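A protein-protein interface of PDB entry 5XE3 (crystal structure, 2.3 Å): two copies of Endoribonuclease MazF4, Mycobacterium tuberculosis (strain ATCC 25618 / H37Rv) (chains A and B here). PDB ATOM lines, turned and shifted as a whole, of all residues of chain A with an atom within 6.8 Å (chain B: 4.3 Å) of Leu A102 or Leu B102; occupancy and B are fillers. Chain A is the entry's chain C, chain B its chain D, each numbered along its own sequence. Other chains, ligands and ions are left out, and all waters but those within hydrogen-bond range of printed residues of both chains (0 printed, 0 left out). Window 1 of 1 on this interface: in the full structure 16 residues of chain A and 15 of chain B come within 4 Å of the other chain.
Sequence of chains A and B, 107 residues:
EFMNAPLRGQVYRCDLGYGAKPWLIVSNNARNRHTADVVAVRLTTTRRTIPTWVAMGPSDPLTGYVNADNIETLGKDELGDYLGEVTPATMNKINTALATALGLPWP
Printed residues of chain B within 4 Å of Leu A102: Arg B8 (2.8 Å), Val B26 (2.9 Å), Val B39 (3.99 Å) and Leu B102 (3.2 Å). Printed residues of chain B within 4 Å of Gly A103: Arg B8 (3.2 Å), Val B26 (3.98 Å) and Asn B28 (3.7 Å). Printed residues of chain B within 4 Å of Leu A104: Arg B8 and Leu B104. Ala B99 touches none of the printed residues of chain A. Of chain A, only Arg A8, Val A26, Val A39, Leu A98 and Leu A102 come within 4 Å of Leu B102. Printed residues of chain A within 4 Å of Gly B103: Arg A8 (3.5 Å).
CD2 of Leu B104 touches NH2 of Arg A8 (3.7 Å). CA of Ser A27 touches O of Ala B101, at 3.7 Å. CD2 of Leu B102 touches CG1 of Val A39, at 3.9 Å. Leu A98 touches Leu B102 (CD2 to CD1, 3.8 Å). Leu B104 touches Leu A98 (CD2 to CB, 3.9 Å). CD1 of Leu B104 touches N of Ala A99, at 3.7 Å. CD1 of Leu A102 touches CD1 of Leu B102 (3.2 Å). Val B26 touches Gly A103 (O to N, 3.98 Å). CA of Gly A103 touches CB of Asn B28, at 3.7 Å. CD1 of Leu B104 touches CD1 of Leu A104, at 3.96 Å.
O of Leu B102 lies close to O of Val A26. The backbone carbonyl oxygen (O) of Val B26 lies close to the backbone carbonyl oxygen (O) of Leu A102 (2.9 Å). The backbone carbonyl oxygen (O) of Gly A103 sits close to the guanidinium group (NE) of Arg B8, 3.3 Å away. O of Ala A101 sits at hydrogen-bond distance from N of Asn B28 (3.2 Å). The backbone carbonyl oxygen (O) of Thr A100 is in hydrogen-bond range of the side-chain amide nitrogen (ND2) of Asn B28 (3.0 Å). The guanidinium group (NH2) of Arg B8 lies within hydrogen-bond range of the backbone carbonyl oxygen (O) of Leu A102, 2.8 Å away. The backbone carbonyl oxygen (O) of Ala B101 sits at hydrogen-bond distance from the backbone NH (N) of Asn A28, at 3.1 Å. NH2 of Arg A8 lies within hydrogen-bond range of O of Leu B102 (2.9 Å). The side-chain amide nitrogen (ND2) of Asn A28 lies within hydrogen-bond range of the backbone carbonyl oxygen (O) of Thr B100, at 3.2 Å.
NE of Arg B8 is in hydrogen-bond range of O of Val B26. The side-chain hydroxyl (OG) of Ser A27 sits at hydrogen-bond distance from the backbone NH (N) of Val A39, 2.8 Å away. O of Ala A99 sits at hydrogen-bond distance from N of Leu A104 (3.0 Å). N of Val B26 is in hydrogen-bond range of O of Val B39, 2.8 Å away. NE of Arg A8 lies within hydrogen-bond range of O of Val A26 (2.9 Å). The backbone NH (N) of Leu B104 sits at hydrogen-bond distance from the backbone carbonyl oxygen (O) of Ala B99 (2.7 Å).
Of the 20 printed residues of chain A, 13 touch a printed residue of chain B. Hydrophobic or aromatic side chains of chain A within 4 Å of the printed part of chain B: Val A26, Val A39, Leu A98, Leu A102 and Leu A104. Printed residues of chain B that touch a printed residue of chain A: Arg B8, Val B26, Asn B28, Val B39, Thr B100, Ala B101, Leu B102, Gly B103 and Leu B104. Hydrophobic or aromatic side chains of chain B that line the printed part of chain A: Val B39, Leu B102 and Leu B104. Among the printed residues, 23 pairs touch across the chains. Among the printed residues, no Asp or Glu carboxylate lies within 4 Å of a Lys or Arg side-chain nitrogen of the other chain.
Arg A8 touches Leu B104, and with the chains exchanged Leu A104 touches Arg B8. Asn A28 touches Thr B100, and with the chains exchanged Thr A100 touches Asn B28. Ala A99 touches Leu B104, but with the chains exchanged Leu A104 does not touch Ala B99 (4.4 Å). Gly A103 touches Val B26, but with the chains exchanged Val A26 does not touch Gly B103 (4.01 Å). 11 positions are printed for both chains. Of the 23 pairs that touch across the chains among the printed residues, 16 have their exchanged pair printed and touching as well.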
ATOM      1  N   ARG A   8      24.458 -17.371   5.280  1.00  0.00           N
ATOM      2  CA  ARG A   8      24.804 -18.756   5.130  1.00  0.00           C
ATOM      3  C   ARG A   8      24.884 -19.096   3.614  1.00  0.00           C
ATOM      4  O   ARG A   8      23.947 -18.814   2.835  1.00  0.00           O
ATOM      5  CB  ARG A   8      23.775 -19.642   5.897  1.00  0.00           C
ATOM      6  CG  ARG A   8      24.238 -21.078   6.044  1.00  0.00           C
ATOM      7  CD  ARG A   8      23.243 -21.974   6.760  1.00  0.00           C
ATOM      8  NE  ARG A   8      23.913 -23.228   7.123  1.00  0.00           N
ATOM      9  CZ  ARG A   8      23.945 -24.340   6.392  1.00  0.00           C
ATOM     10  NH1 ARG A   8      23.332 -24.407   5.222  1.00  0.00           N
ATOM     11  NH2 ARG A   8      24.592 -25.415   6.843  1.00  0.00           N
ATOM     12  N   VAL A  26      28.572 -21.140   7.685  1.00  0.00           N
ATOM     13  CA  VAL A  26      27.575 -22.181   7.971  1.00  0.00           C
ATOM     14  C   VAL A  26      26.660 -21.804   9.136  1.00  0.00           C
ATOM     15  O   VAL A  26      25.590 -22.390   9.276  1.00  0.00           O
ATOM     16  CB  VAL A  26      28.243 -23.559   8.228  1.00  0.00           C
ATOM     17  CG1 VAL A  26      28.990 -24.061   6.976  1.00  0.00           C
ATOM     18  CG2 VAL A  26      29.221 -23.518   9.393  1.00  0.00           C
ATOM     19  N   SER A  27      27.075 -20.891  10.007  1.00  0.00           N
ATOM     20  CA  SER A  27      26.133 -20.253  10.972  1.00  0.00           C
ATOM     21  C   SER A  27      24.786 -19.877  10.367  1.00  0.00           C
ATOM     22  O   SER A  27      24.771 -19.392   9.254  1.00  0.00           O
ATOM     23  CB  SER A  27      26.733 -18.934  11.413  1.00  0.00           C
ATOM     24  OG  SER A  27      27.579 -19.130  12.461  1.00  0.00           O
ATOM     25  N   ASN A  28      23.678 -20.037  11.081  1.00  0.00           N
ATOM     26  CA  ASN A  28      22.388 -19.554  10.543  1.00  0.00           C
ATOM     27  C   ASN A  28      22.301 -18.033  10.492  1.00  0.00           C
ATOM     28  O   ASN A  28      23.019 -17.351  11.222  1.00  0.00           O
ATOM     29  CB  ASN A  28      21.171 -20.087  11.328  1.00  0.00           C
ATOM     30  CG  ASN A  28      20.991 -19.405  12.679  1.00  0.00           C
ATOM     31  OD1 ASN A  28      20.794 -18.179  12.768  1.00  0.00           O
ATOM     32  ND2 ASN A  28      21.055 -20.191  13.736  1.00  0.00           N
ATOM     33  N   VAL A  39      30.285 -18.546  12.183  1.00  0.00           N
ATOM     34  CA  VAL A  39      30.900 -19.844  12.097  1.00  0.00           C
ATOM     35  C   VAL A  39      31.045 -20.191  10.618  1.00  0.00           C
ATOM     36  O   VAL A  39      30.101 -20.078   9.845  1.00  0.00           O
ATOM     37  CB  VAL A  39      30.095 -20.931  12.858  1.00  0.00           C
ATOM     38  CG1 VAL A  39      30.857 -22.264  12.873  1.00  0.00           C
ATOM     39  CG2 VAL A  39      29.826 -20.503  14.303  1.00  0.00           C
ATOM     40  N   ALA A  40      32.240 -20.663  10.261  1.00  0.00           N
ATOM     41  CA  ALA A  40      32.563 -20.962   8.909  1.00  0.00           C
ATOM     42  C   ALA A  40      33.412 -22.236   8.801  1.00  0.00           C
ATOM     43  O   ALA A  40      33.976 -22.666   9.787  1.00  0.00           O
ATOM     44  CB  ALA A  40      33.279 -19.779   8.296  1.00  0.00           C
ATOM     45  N   THR A  52      33.469 -36.065   5.270  1.00  0.00           N
ATOM     46  CA  THR A  52      33.387 -34.668   5.717  1.00  0.00           C
ATOM     47  C   THR A  52      33.848 -33.612   4.706  1.00  0.00           C
ATOM     48  O   THR A  52      33.734 -32.386   4.957  1.00  0.00           O
ATOM     49  CB  THR A  52      34.123 -34.473   7.041  1.00  0.00           C
ATOM     50  OG1 THR A  52      35.422 -35.093   6.996  1.00  0.00           O
ATOM     51  CG2 THR A  52      33.315 -35.100   8.167  1.00  0.00           C
ATOM     52  N   ALA A  68      34.622 -29.919   6.480  1.00  0.00           N
ATOM     53  CA  ALA A  68      33.657 -29.621   7.549  1.00  0.00           C
ATOM     54  C   ALA A  68      34.166 -30.060   8.900  1.00  0.00           C
ATOM     55  O   ALA A  68      33.520 -29.796   9.909  1.00  0.00           O
ATOM     56  CB  ALA A  68      32.303 -30.266   7.246  1.00  0.00           C
ATOM     57  N   ASP A  69      35.327 -30.729   8.955  1.00  0.00           N
ATOM     58  CA  ASP A  69      35.948 -30.998  10.231  1.00  0.00           C
ATOM     59  C   ASP A  69      36.629 -29.771  10.818  1.00  0.00           C
ATOM     60  O   ASP A  69      37.024 -29.803  11.949  1.00  0.00           O
ATOM     61  CB  ASP A  69      36.979 -32.109  10.113  1.00  0.00           C
ATOM     62  CG  ASP A  69      36.352 -33.489  10.001  1.00  0.00           C
ATOM     63  OD1 ASP A  69      35.660 -33.905  10.979  1.00  0.00           O
ATOM     64  OD2 ASP A  69      36.588 -34.167   8.951  1.00  0.00           O
ATOM     65  N   ILE A  71      35.951 -26.356  11.554  1.00  0.00           N
ATOM     66  CA  ILE A  71      35.004 -25.278  11.834  1.00  0.00           C
ATOM     67  C   ILE A  71      35.699 -24.176  12.650  1.00  0.00           C
ATOM     68  O   ILE A  71      36.452 -24.460  13.523  1.00  0.00           O
ATOM     69  CB  ILE A  71      33.804 -25.859  12.599  1.00  0.00           C
ATOM     70  CG1 ILE A  71      33.093 -26.911  11.730  1.00  0.00           C
ATOM     71  CG2 ILE A  71      32.810 -24.777  12.989  1.00  0.00           C
ATOM     72  CD1 ILE A  71      32.687 -28.118  12.524  1.00  0.00           C
ATOM     73  N   ASN A  95      25.743 -29.706   4.246  1.00  0.00           N
ATOM     74  CA  ASN A  95      24.899 -30.031   5.387  1.00  0.00           C
ATOM     75  C   ASN A  95      25.183 -31.433   5.890  1.00  0.00           C
ATOM     76  O   ASN A  95      25.484 -31.618   7.050  1.00  0.00           O
ATOM     77  CB  ASN A  95      23.440 -29.883   5.015  1.00  0.00           C
ATOM     78  CG  ASN A  95      23.082 -28.460   4.719  1.00  0.00           C
ATOM     79  OD1 ASN A  95      23.830 -27.539   5.056  1.00  0.00           O
ATOM     80  ND2 ASN A  95      21.952 -28.262   4.086  1.00  0.00           N
ATOM     81  N   ALA A  97      27.834 -33.261   5.303  1.00  0.00           N
ATOM     82  CA  ALA A  97      29.188 -33.351   5.788  1.00  0.00           C
ATOM     83  C   ALA A  97      29.301 -32.796   7.198  1.00  0.00           C
ATOM     84  O   ALA A  97      30.000 -33.345   8.019  1.00  0.00           O
ATOM     85  CB  ALA A  97      30.146 -32.627   4.831  1.00  0.00           C
ATOM     86  N   LEU A  98      28.669 -31.663   7.436  1.00  0.00           N
ATOM     87  CA  LEU A  98      28.643 -31.063   8.749  1.00  0.00           C
ATOM     88  C   LEU A  98      27.987 -31.969   9.785  1.00  0.00           C
ATOM     89  O   LEU A  98      28.519 -32.169  10.864  1.00  0.00           O
ATOM     90  CB  LEU A  98      27.900 -29.732   8.707  1.00  0.00           C
ATOM     91  CG  LEU A  98      28.769 -28.486   8.610  1.00  0.00           C
ATOM     92  CD1 LEU A  98      27.910 -27.293   8.252  1.00  0.00           C
ATOM     93  CD2 LEU A  98      29.477 -28.292   9.940  1.00  0.00           C
ATOM     94  N   ALA A  99      26.820 -32.488   9.449  1.00  0.00           N
ATOM     95  CA  ALA A  99      26.077 -33.318  10.373  1.00  0.00           C
ATOM     96  C   ALA A  99      26.969 -34.491  10.743  1.00  0.00           C
ATOM     97  O   ALA A  99      27.105 -34.847  11.915  1.00  0.00           O
ATOM     98  CB  ALA A  99      24.772 -33.800   9.728  1.00  0.00           C
ATOM     99  N   THR A 100      27.614 -35.065   9.747  1.00  0.00           N
ATOM    100  CA  THR A 100      28.568 -36.126  10.005  1.00  0.00           C
ATOM    101  C   THR A 100      29.700 -35.732  10.915  1.00  0.00           C
ATOM    102  O   THR A 100      30.037 -36.473  11.808  1.00  0.00           O
ATOM    103  CB  THR A 100      29.190 -36.586   8.705  1.00  0.00           C
ATOM    104  OG1 THR A 100      28.161 -37.213   7.964  1.00  0.00           O
ATOM    105  CG2 THR A 100      30.331 -37.580   8.933  1.00  0.00           C
ATOM    106  N   ALA A 101      30.315 -34.599  10.651  1.00  0.00           N
ATOM    107  CA  ALA A 101      31.398 -34.100  11.496  1.00  0.00           C
ATOM    108  C   ALA A 101      30.984 -33.873  12.956  1.00  0.00           C
ATOM    109  O   ALA A 101      31.776 -34.101  13.871  1.00  0.00           O
ATOM    110  CB  ALA A 101      31.959 -32.805  10.923  1.00  0.00           C
ATOM    111  N   LEU A 102      29.762 -33.429  13.172  1.00  0.00           N
ATOM    112  CA  LEU A 102      29.269 -33.200  14.525  1.00  0.00           C
ATOM    113  C   LEU A 102      28.421 -34.338  15.031  1.00  0.00           C
ATOM    114  O   LEU A 102      27.608 -34.121  15.945  1.00  0.00           O
ATOM    115  CB  LEU A 102      28.453 -31.915  14.577  1.00  0.00           C
ATOM    116  CG  LEU A 102      29.299 -30.718  14.226  1.00  0.00           C
ATOM    117  CD1 LEU A 102      28.415 -29.525  14.230  1.00  0.00           C
ATOM    118  CD2 LEU A 102      30.461 -30.528  15.210  1.00  0.00           C
ATOM    119  N   GLY A 103      28.593 -35.523  14.426  1.00  0.00           N
ATOM    120  CA  GLY A 103      28.018 -36.768  14.881  1.00  0.00           C
ATOM    121  C   GLY A 103      26.527 -36.765  15.113  1.00  0.00           C
ATOM    122  O   GLY A 103      26.041 -37.361  16.055  1.00  0.00           O
ATOM    123  N   LEU A 104      25.786 -36.075  14.278  1.00  0.00           N
ATOM    124  CA  LEU A 104      24.348 -36.182  14.334  1.00  0.00           C
ATOM    125  C   LEU A 104      23.922 -37.637  14.035  1.00  0.00           C
ATOM    126  O   LEU A 104      24.488 -38.272  13.158  1.00  0.00           O
ATOM    127  CB  LEU A 104      23.702 -35.186  13.386  1.00  0.00           C
ATOM    128  CG  LEU A 104      24.046 -33.736  13.726  1.00  0.00           C
ATOM    129  CD1 LEU A 104      23.128 -32.855  12.913  1.00  0.00           C
ATOM    130  CD2 LEU A 104      23.910 -33.400  15.202  1.00  0.00           C
ATOM    131  N   PRO A 105      22.963 -38.176  14.826  1.00  0.00           N
ATOM    132  CA  PRO A 105      22.632 -39.602  14.693  1.00  0.00           C
ATOM    133  C   PRO A 105      21.824 -39.930  13.444  1.00  0.00           C
ATOM    134  O   PRO A 105      21.240 -39.060  12.806  1.00  0.00           O
ATOM    135  CB  PRO A 105      21.826 -39.912  15.985  1.00  0.00           C
ATOM    136  CG  PRO A 105      21.280 -38.594  16.436  1.00  0.00           C
ATOM    137  CD  PRO A 105      22.290 -37.555  15.998  1.00  0.00           C
ATOM    138  N   ARG B   8      31.416 -38.654  22.223  1.00  0.00           N
ATOM    139  CA  ARG B   8      30.350 -37.702  22.062  1.00  0.00           C
ATOM    140  C   ARG B   8      29.321 -37.805  23.217  1.00  0.00           C
ATOM    141  O   ARG B   8      28.906 -38.873  23.549  1.00  0.00           O
ATOM    142  CB  ARG B   8      29.655 -38.007  20.720  1.00  0.00           C
ATOM    143  CG  ARG B   8      28.656 -36.962  20.331  1.00  0.00           C
ATOM    144  CD  ARG B   8      28.162 -37.089  18.931  1.00  0.00           C
ATOM    145  NE  ARG B   8      27.561 -35.836  18.510  1.00  0.00           N
ATOM    146  CZ  ARG B   8      26.301 -35.463  18.669  1.00  0.00           C
ATOM    147  NH1 ARG B   8      25.425 -36.228  19.295  1.00  0.00           N
ATOM    148  NH2 ARG B   8      25.903 -34.289  18.170  1.00  0.00           N
ATOM    149  N   VAL B  26      30.920 -32.824  21.151  1.00  0.00           N
ATOM    150  CA  VAL B  26      29.903 -32.961  20.073  1.00  0.00           C
ATOM    151  C   VAL B  26      30.466 -33.557  18.780  1.00  0.00           C
ATOM    152  O   VAL B  26      29.724 -33.993  17.925  1.00  0.00           O
ATOM    153  CB  VAL B  26      29.184 -31.627  19.808  1.00  0.00           C
ATOM    154  CG1 VAL B  26      28.389 -31.149  21.038  1.00  0.00           C
ATOM    155  CG2 VAL B  26      30.178 -30.543  19.455  1.00  0.00           C
ATOM    156  N   ASN B  28      32.038 -36.316  16.173  1.00  0.00           N
ATOM    157  CA  ASN B  28      31.771 -37.734  16.033  1.00  0.00           C
ATOM    158  C   ASN B  28      32.940 -38.540  16.594  1.00  0.00           C
ATOM    159  O   ASN B  28      34.086 -38.022  16.695  1.00  0.00           O
ATOM    160  CB  ASN B  28      31.455 -38.069  14.570  1.00  0.00           C
ATOM    161  CG  ASN B  28      32.690 -38.058  13.704  1.00  0.00           C
ATOM    162  OD1 ASN B  28      33.597 -38.864  13.904  1.00  0.00           O
ATOM    163  ND2 ASN B  28      32.748 -37.148  12.762  1.00  0.00           N
ATOM    164  N   VAL B  39      35.752 -31.539  19.264  1.00  0.00           N
ATOM    165  CA  VAL B  39      34.955 -30.318  19.186  1.00  0.00           C
ATOM    166  C   VAL B  39      33.945 -30.363  20.335  1.00  0.00           C
ATOM    167  O   VAL B  39      33.261 -31.361  20.530  1.00  0.00           O
ATOM    168  CB  VAL B  39      34.192 -30.290  17.843  1.00  0.00           C
ATOM    169  CG1 VAL B  39      33.219 -29.122  17.724  1.00  0.00           C
ATOM    170  CG2 VAL B  39      35.172 -30.258  16.672  1.00  0.00           C
ATOM    171  N   LEU B  98      22.407 -27.805  17.900  1.00  0.00           N
ATOM    172  CA  LEU B  98      23.532 -27.793  16.950  1.00  0.00           C
ATOM    173  C   LEU B  98      23.052 -27.587  15.511  1.00  0.00           C
ATOM    174  O   LEU B  98      23.616 -26.773  14.772  1.00  0.00           O
ATOM    175  CB  LEU B  98      24.340 -29.081  17.037  1.00  0.00           C
ATOM    176  CG  LEU B  98      25.313 -29.184  18.185  1.00  0.00           C
ATOM    177  CD1 LEU B  98      25.924 -30.579  18.210  1.00  0.00           C
ATOM    178  CD2 LEU B  98      26.409 -28.156  18.051  1.00  0.00           C
ATOM    179  N   ALA B  99      21.993 -28.280  15.121  1.00  0.00           N
ATOM    180  CA  ALA B  99      21.466 -28.171  13.730  1.00  0.00           C
ATOM    181  C   ALA B  99      20.766 -26.839  13.435  1.00  0.00           C
ATOM    182  O   ALA B  99      20.887 -26.270  12.327  1.00  0.00           O
ATOM    183  CB  ALA B  99      20.551 -29.329  13.418  1.00  0.00           C
ATOM    184  N   THR B 100      20.039 -26.325  14.420  1.00  0.00           N
ATOM    185  CA  THR B 100      19.572 -24.952  14.337  1.00  0.00           C
ATOM    186  C   THR B 100      20.805 -24.022  14.238  1.00  0.00           C
ATOM    187  O   THR B 100      20.957 -23.323  13.278  1.00  0.00           O
ATOM    188  CB  THR B 100      18.668 -24.588  15.537  1.00  0.00           C
ATOM    189  OG1 THR B 100      17.502 -25.445  15.550  1.00  0.00           O
ATOM    190  CG2 THR B 100      18.237 -23.123  15.466  1.00  0.00           C
ATOM    191  N   ALA B 101      21.716 -24.047  15.203  1.00  0.00           N
ATOM    192  CA  ALA B 101      22.884 -23.160  15.176  1.00  0.00           C
ATOM    193  C   ALA B 101      23.665 -23.128  13.833  1.00  0.00           C
ATOM    194  O   ALA B 101      24.100 -22.063  13.407  1.00  0.00           O
ATOM    195  CB  ALA B 101      23.836 -23.516  16.296  1.00  0.00           C
ATOM    196  N   LEU B 102      23.815 -24.283  13.191  1.00  0.00           N
ATOM    197  CA  LEU B 102      24.547 -24.431  11.939  1.00  0.00           C
ATOM    198  C   LEU B 102      23.665 -24.614  10.696  1.00  0.00           C
ATOM    199  O   LEU B 102      24.144 -25.075   9.643  1.00  0.00           O
ATOM    200  CB  LEU B 102      25.490 -25.632  12.059  1.00  0.00           C
ATOM    201  CG  LEU B 102      26.685 -25.498  12.984  1.00  0.00           C
ATOM    202  CD1 LEU B 102      27.537 -26.758  12.841  1.00  0.00           C
ATOM    203  CD2 LEU B 102      27.524 -24.311  12.644  1.00  0.00           C
ATOM    204  N   GLY B 103      22.392 -24.262  10.796  1.00  0.00           N
ATOM    205  CA  GLY B 103      21.463 -24.388   9.659  1.00  0.00           C
ATOM    206  C   GLY B 103      21.329 -25.741   8.969  1.00  0.00           C
ATOM    207  O   GLY B 103      21.078 -25.794   7.774  1.00  0.00           O
ATOM    208  N   LEU B 104      21.472 -26.821   9.733  1.00  0.00           N
ATOM    209  CA  LEU B 104      21.294 -28.170   9.230  1.00  0.00           C
ATOM    210  C   LEU B 104      19.827 -28.607   9.256  1.00  0.00           C
ATOM    211  O   LEU B 104      19.028 -28.091  10.037  1.00  0.00           O
ATOM    212  CB  LEU B 104      22.177 -29.157  10.010  1.00  0.00           C
ATOM    213  CG  LEU B 104      23.678 -28.808  10.048  1.00  0.00           C
ATOM    214  CD1 LEU B 104      24.543 -29.834  10.784  1.00  0.00           C
ATOM    215  CD2 LEU B 104      24.199 -28.606   8.637  1.00  0.00           C
